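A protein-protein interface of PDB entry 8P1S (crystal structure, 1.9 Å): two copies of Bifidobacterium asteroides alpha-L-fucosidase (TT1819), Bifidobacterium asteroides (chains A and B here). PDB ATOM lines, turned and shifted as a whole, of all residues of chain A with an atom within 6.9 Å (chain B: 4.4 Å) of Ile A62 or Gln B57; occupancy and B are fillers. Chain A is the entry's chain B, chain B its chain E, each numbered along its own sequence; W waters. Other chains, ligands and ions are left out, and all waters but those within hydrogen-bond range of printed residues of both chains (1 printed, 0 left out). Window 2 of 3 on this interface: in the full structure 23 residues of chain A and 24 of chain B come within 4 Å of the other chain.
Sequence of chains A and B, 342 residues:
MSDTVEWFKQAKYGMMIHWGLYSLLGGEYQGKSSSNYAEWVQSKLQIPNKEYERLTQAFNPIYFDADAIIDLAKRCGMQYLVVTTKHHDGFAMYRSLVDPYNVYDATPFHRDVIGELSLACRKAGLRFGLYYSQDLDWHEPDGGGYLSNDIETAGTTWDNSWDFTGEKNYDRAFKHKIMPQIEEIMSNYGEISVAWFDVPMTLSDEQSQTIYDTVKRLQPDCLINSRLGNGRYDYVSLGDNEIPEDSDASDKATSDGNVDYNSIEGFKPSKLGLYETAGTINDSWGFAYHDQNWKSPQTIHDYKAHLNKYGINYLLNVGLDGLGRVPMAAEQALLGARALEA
Of the 7 printed residues of chain B, 4 touch a printed residue of chain A. Hydrophobic or aromatic side chains of chain B that line the printed part of chain A: Leu B55 and Ala B58. Among the printed residues, no Asp or Glu carboxylate lies within 4 Å of a Lys or Arg side-chain nitrogen of the other chain.
The backbone NH (N) of Tyr A63 lies within hydrogen-bond range of the backbone carbonyl oxygen (O) of Leu A323, 3.0 Å away. O of Leu A323 sits at hydrogen-bond distance from N of Phe A64, at 3.3 Å.
Water W1 lies within hydrogen-bond range of the side-chain amide oxygen of Gln B57 (2.8 Å) and the side-chain amide nitrogen of Asn A60 (3.1 Å).
Position printed for both chains: 108.
Among the printed residues, pairs that only touch across the chains: Ile A62 with Arg B54, Tyr A63 with Leu B55, Ile A62 with Gln B57, Asn A60 with Ala B58, Leu A323 with Ala B58 and Ile A62 with Leu B55.
Gln B57 touches two residues of chain A. Printed residues of chain B within 4 Å of Asn A60: Gln B57 (3.0 Å) and Ala B58 (3.8 Å). Of the printed residues of chain A, Leu B55 touches Ile A62 and Tyr A63. Printed residues of chain B within 4 Å of Tyr A63: Leu B55 (3.6 Å). Printed residues of chain A within 4 Å of Arg B54: Ile A62 (3.5 Å). Of the printed residues of chain A, Ala B58 touches Asn A60 (3.8 Å) and Leu A323 (3.9 Å). Phe A64 touches none of the printed residues of chain B. The nearest residue of chain A that does not touch Gln B57 is Pro A108 (6.8 Å). The nearest printed residue of chain A that does not touch Ala B58 is Ile A62 (4.4 Å).
ND2 of Asn A60 is in hydrogen-bond range of O of Gln B57, at 3.0 Å.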
ATOM      1  N   ASN A  60       0.031  28.065  26.977  1.00  0.00           N
ATOM      2  CA  ASN A  60      -1.400  27.856  27.157  1.00  0.00           C
ATOM      3  C   ASN A  60      -1.710  26.345  27.138  1.00  0.00           C
ATOM      4  O   ASN A  60      -2.333  25.827  26.214  1.00  0.00           O
ATOM      5  CB  ASN A  60      -2.244  28.620  26.165  1.00  0.00           C
ATOM      6  CG  ASN A  60      -3.695  28.567  26.627  1.00  0.00           C
ATOM      7  OD1 ASN A  60      -3.941  28.309  27.817  1.00  0.00           O
ATOM      8  ND2 ASN A  60      -4.663  28.582  25.693  1.00  0.00           N
ATOM      9  N   PRO A  61      -1.253  25.632  28.163  1.00  0.00           N
ATOM     10  CA  PRO A  61      -1.380  24.172  28.211  1.00  0.00           C
ATOM     11  C   PRO A  61      -2.773  23.675  28.545  1.00  0.00           C
ATOM     12  O   PRO A  61      -3.077  23.308  29.666  1.00  0.00           O
ATOM     13  CB  PRO A  61      -0.378  23.784  29.298  1.00  0.00           C
ATOM     14  CG  PRO A  61      -0.406  24.968  30.223  1.00  0.00           C
ATOM     15  CD  PRO A  61      -0.511  26.185  29.328  1.00  0.00           C
ATOM     16  N   ILE A  62      -3.575  23.556  27.481  1.00  0.00           N
ATOM     17  CA  ILE A  62      -4.983  23.279  27.609  1.00  0.00           C
ATOM     18  C   ILE A  62      -5.222  21.880  28.191  1.00  0.00           C
ATOM     19  O   ILE A  62      -6.357  21.591  28.490  1.00  0.00           O
ATOM     20  CB  ILE A  62      -5.682  23.436  26.260  1.00  0.00           C
ATOM     21  CG1 ILE A  62      -5.091  22.536  25.169  1.00  0.00           C
ATOM     22  CG2 ILE A  62      -5.681  24.908  25.837  1.00  0.00           C
ATOM     23  CD1 ILE A  62      -5.996  22.394  23.889  1.00  0.00           C
ATOM     24  N   TYR A  63      -4.261  20.944  28.183  1.00  0.00           N
ATOM     25  CA  TYR A  63      -4.534  19.590  28.669  1.00  0.00           C
ATOM     26  C   TYR A  63      -4.013  19.424  30.108  1.00  0.00           C
ATOM     27  O   TYR A  63      -4.128  18.364  30.690  1.00  0.00           O
ATOM     28  CB  TYR A  63      -3.932  18.531  27.748  1.00  0.00           C
ATOM     29  CG  TYR A  63      -4.583  18.517  26.394  1.00  0.00           C
ATOM     30  CD1 TYR A  63      -5.923  18.216  26.270  1.00  0.00           C
ATOM     31  CD2 TYR A  63      -3.920  18.859  25.260  1.00  0.00           C
ATOM     32  CE1 TYR A  63      -6.585  18.236  25.048  1.00  0.00           C
ATOM     33  CE2 TYR A  63      -4.539  18.882  24.008  1.00  0.00           C
ATOM     34  CZ  TYR A  63      -5.891  18.586  23.904  1.00  0.00           C
ATOM     35  OH  TYR A  63      -6.598  18.611  22.738  1.00  0.00           O
ATOM     36  N   PHE A  64      -3.519  20.484  30.757  1.00  0.00           N
ATOM     37  CA  PHE A  64      -3.064  20.340  32.144  1.00  0.00           C
ATOM     38  C   PHE A  64      -4.255  20.001  33.033  1.00  0.00           C
ATOM     39  O   PHE A  64      -5.286  20.685  33.044  1.00  0.00           O
ATOM     40  CB  PHE A  64      -2.418  21.633  32.669  1.00  0.00           C
ATOM     41  CG  PHE A  64      -1.946  21.525  34.088  1.00  0.00           C
ATOM     42  CD1 PHE A  64      -0.897  20.688  34.421  1.00  0.00           C
ATOM     43  CD2 PHE A  64      -2.562  22.261  35.100  1.00  0.00           C
ATOM     44  CE1 PHE A  64      -0.463  20.604  35.735  1.00  0.00           C
ATOM     45  CE2 PHE A  64      -2.125  22.154  36.424  1.00  0.00           C
ATOM     46  CZ  PHE A  64      -1.089  21.301  36.736  1.00  0.00           C
ATOM     47  N   ASP A  65      -4.121  18.924  33.786  1.00  0.00           N
ATOM     48  CA  ASP A  65      -5.165  18.517  34.710  1.00  0.00           C
ATOM     49  C   ASP A  65      -4.537  17.967  36.005  1.00  0.00           C
ATOM     50  O   ASP A  65      -4.068  16.828  36.051  1.00  0.00           O
ATOM     51  CB  ASP A  65      -6.097  17.526  34.056  1.00  0.00           C
ATOM     52  CG  ASP A  65      -7.241  17.072  34.973  1.00  0.00           C
ATOM     53  OD1 ASP A  65      -7.210  17.291  36.198  1.00  0.00           O
ATOM     54  OD2 ASP A  65      -8.162  16.470  34.452  1.00  0.00           O
ATOM     55  N   PRO A 108      -1.022  33.623  29.083  1.00  0.00           N
ATOM     56  CA  PRO A 108      -2.454  33.573  28.841  1.00  0.00           C
ATOM     57  C   PRO A 108      -3.079  32.493  29.729  1.00  0.00           C
ATOM     58  O   PRO A 108      -4.253  32.562  29.981  1.00  0.00           O
ATOM     59  CB  PRO A 108      -2.644  33.284  27.339  1.00  0.00           C
ATOM     60  CG  PRO A 108      -1.245  33.162  26.756  1.00  0.00           C
ATOM     61  CD  PRO A 108      -0.212  33.348  27.878  1.00  0.00           C
ATOM     62  N   PHE A 109      -2.330  31.486  30.177  1.00  0.00           N
ATOM     63  CA  PHE A 109      -2.941  30.431  30.989  1.00  0.00           C
ATOM     64  C   PHE A 109      -3.523  31.008  32.287  1.00  0.00           C
ATOM     65  O   PHE A 109      -4.568  30.584  32.732  1.00  0.00           O
ATOM     66  CB  PHE A 109      -1.863  29.395  31.288  1.00  0.00           C
ATOM     67  CG  PHE A 109      -2.359  28.076  31.838  1.00  0.00           C
ATOM     68  CD1 PHE A 109      -3.275  27.327  31.156  1.00  0.00           C
ATOM     69  CD2 PHE A 109      -1.840  27.565  33.019  1.00  0.00           C
ATOM     70  CE1 PHE A 109      -3.735  26.110  31.642  1.00  0.00           C
ATOM     71  CE2 PHE A 109      -2.258  26.345  33.510  1.00  0.00           C
ATOM     72  CZ  PHE A 109      -3.192  25.629  32.812  1.00  0.00           C
ATOM     73  N   ARG A 111      -3.184  30.840  35.512  1.00  0.00           N
ATOM     74  CA  ARG A 111      -3.546  29.914  36.549  1.00  0.00           C
ATOM     75  C   ARG A 111      -2.312  29.590  37.396  1.00  0.00           C
ATOM     76  O   ARG A 111      -1.210  29.570  36.912  1.00  0.00           O
ATOM     77  CB  ARG A 111      -4.132  28.641  35.943  1.00  0.00           C
ATOM     78  CG  ARG A 111      -5.580  28.791  35.422  1.00  0.00           C
ATOM     79  CD  ARG A 111      -6.047  27.757  34.392  1.00  0.00           C
ATOM     80  NE  ARG A 111      -5.886  26.404  34.917  1.00  0.00           N
ATOM     81  CZ  ARG A 111      -6.153  25.298  34.231  1.00  0.00           C
ATOM     82  NH1 ARG A 111      -6.687  25.402  33.038  1.00  0.00           N
ATOM     83  NH2 ARG A 111      -5.987  24.089  34.769  1.00  0.00           N
ATOM     84  N   GLY A 322       4.500  20.702  26.677  1.00  0.00           N
ATOM     85  CA  GLY A 322       4.058  22.089  26.490  1.00  0.00           C
ATOM     86  C   GLY A 322       2.554  22.239  26.608  1.00  0.00           C
ATOM     87  O   GLY A 322       2.054  23.338  26.784  1.00  0.00           O
ATOM     88  N   LEU A 323       1.812  21.118  26.495  1.00  0.00           N
ATOM     89  CA  LEU A 323       0.369  21.155  26.644  1.00  0.00           C
ATOM     90  C   LEU A 323      -0.084  20.728  28.049  1.00  0.00           C
ATOM     91  O   LEU A 323      -1.279  20.698  28.319  1.00  0.00           O
ATOM     92  CB  LEU A 323      -0.238  20.248  25.591  1.00  0.00           C
ATOM     93  CG  LEU A 323      -0.151  20.740  24.151  1.00  0.00           C
ATOM     94  CD1 LEU A 323      -0.592  19.636  23.227  1.00  0.00           C
ATOM     95  CD2 LEU A 323      -0.955  22.008  23.935  1.00  0.00           C
ATOM     96  N   GLY A 324       0.872  20.470  28.920  1.00  0.00           N
ATOM     97  CA  GLY A 324       0.630  20.124  30.311  1.00  0.00           C
ATOM     98  C   GLY A 324       0.388  18.629  30.521  1.00  0.00           C
ATOM     99  O   GLY A 324      -0.129  18.237  31.562  1.00  0.00           O
ATOM    100  N   ARG B  54     -10.479  22.576  20.369  1.00  0.00           N
ATOM    101  CA  ARG B  54      -9.899  23.270  21.506  1.00  0.00           C
ATOM    102  C   ARG B  54      -8.408  23.558  21.212  1.00  0.00           C
ATOM    103  O   ARG B  54      -7.878  24.512  21.751  1.00  0.00           O
ATOM    104  CB  ARG B  54     -10.081  22.459  22.781  1.00  0.00           C
ATOM    105  CG  ARG B  54     -11.512  22.300  23.266  1.00  0.00           C
ATOM    106  CD  ARG B  54     -11.571  21.485  24.553  1.00  0.00           C
ATOM    107  NE  ARG B  54     -10.918  22.325  25.576  1.00  0.00           N
ATOM    108  CZ  ARG B  54      -9.876  22.007  26.383  1.00  0.00           C
ATOM    109  NH1 ARG B  54      -9.408  20.765  26.479  1.00  0.00           N
ATOM    110  NH2 ARG B  54      -9.350  22.963  27.142  1.00  0.00           N
ATOM    111  N   LEU B  55      -7.753  22.741  20.367  1.00  0.00           N
ATOM    112  CA  LEU B  55      -6.355  22.986  19.959  1.00  0.00           C
ATOM    113  C   LEU B  55      -6.129  24.388  19.382  1.00  0.00           C
ATOM    114  O   LEU B  55      -5.020  24.917  19.500  1.00  0.00           O
ATOM    115  CB  LEU B  55      -5.900  21.926  18.966  1.00  0.00           C
ATOM    116  CG  LEU B  55      -5.786  20.498  19.567  1.00  0.00           C
ATOM    117  CD1 LEU B  55      -5.773  19.450  18.469  1.00  0.00           C
ATOM    118  CD2 LEU B  55      -4.532  20.373  20.371  1.00  0.00           C
ATOM    119  N   THR B  56      -7.154  24.972  18.757  1.00  0.00           N
ATOM    120  CA  THR B  56      -6.995  26.327  18.213  1.00  0.00           C
ATOM    121  C   THR B  56      -6.510  27.292  19.285  1.00  0.00           C
ATOM    122  O   THR B  56      -5.735  28.206  18.973  1.00  0.00           O
ATOM    123  CB  THR B  56      -8.285  26.885  17.572  1.00  0.00           C
ATOM    124  OG1 THR B  56      -9.290  26.927  18.595  1.00  0.00           O
ATOM    125  CG2 THR B  56      -8.747  26.035  16.416  1.00  0.00           C
ATOM    126  N   GLN B  57      -6.925  27.082  20.534  1.00  0.00           N
ATOM    127  CA  GLN B  57      -6.602  28.046  21.594  1.00  0.00           C
ATOM    128  C   GLN B  57      -5.150  27.885  22.022  1.00  0.00           C
ATOM    129  O   GLN B  57      -4.602  28.739  22.661  1.00  0.00           O
ATOM    130  CB  GLN B  57      -7.480  27.877  22.835  1.00  0.00           C
ATOM    131  CG  GLN B  57      -8.997  27.791  22.667  1.00  0.00           C
ATOM    132  CD  GLN B  57      -9.625  26.778  23.672  1.00  0.00           C
ATOM    133  OE1 GLN B  57      -9.024  26.292  24.650  1.00  0.00           O
ATOM    134  NE2 GLN B  57     -10.874  26.359  23.456  1.00  0.00           N
ATOM    135  N   ALA B  58      -4.506  26.774  21.717  1.00  0.00           N
ATOM    136  CA  ALA B  58      -3.086  26.560  22.051  1.00  0.00           C
ATOM    137  C   ALA B  58      -2.179  26.875  20.862  1.00  0.00           C
ATOM    138  O   ALA B  58      -0.982  26.724  20.973  1.00  0.00           O
ATOM    139  CB  ALA B  58      -2.818  25.137  22.493  1.00  0.00           C
ATOM    140  N   PHE B  59      -2.756  27.256  19.688  1.00  0.00           N
ATOM    141  CA  PHE B  59      -1.980  27.489  18.480  1.00  0.00           C
ATOM    142  C   PHE B  59      -1.417  28.917  18.424  1.00  0.00           C
ATOM    143  O   PHE B  59      -2.099  29.836  17.962  1.00  0.00           O
ATOM    144  CB  PHE B  59      -2.791  27.147  17.242  1.00  0.00           C
ATOM    145  CG  PHE B  59      -1.921  26.963  16.022  1.00  0.00           C
ATOM    146  CD1 PHE B  59      -1.430  25.711  15.685  1.00  0.00           C
ATOM    147  CD2 PHE B  59      -1.667  28.046  15.175  1.00  0.00           C
ATOM    148  CE1 PHE B  59      -0.670  25.564  14.557  1.00  0.00           C
ATOM    149  CE2 PHE B  59      -0.900  27.882  14.039  1.00  0.00           C
ATOM    150  CZ  PHE B  59      -0.363  26.665  13.764  1.00  0.00           C
ATOM    151  N   PRO B 108      -5.116  32.437  18.306  1.00  0.00           N
ATOM    152  CA  PRO B 108      -4.444  33.672  18.736  1.00  0.00           C
ATOM    153  C   PRO B 108      -3.337  34.017  17.764  1.00  0.00           C
ATOM    154  O   PRO B 108      -2.965  35.153  17.710  1.00  0.00           O
ATOM    155  CB  PRO B 108      -3.824  33.376  20.132  1.00  0.00           C
ATOM    156  CG  PRO B 108      -4.196  31.923  20.472  1.00  0.00           C
ATOM    157  CD  PRO B 108      -4.976  31.339  19.285  1.00  0.00           C
HETATM  158  O   HOH W   1      -7.647  28.176  26.216  1.00  0.00           O
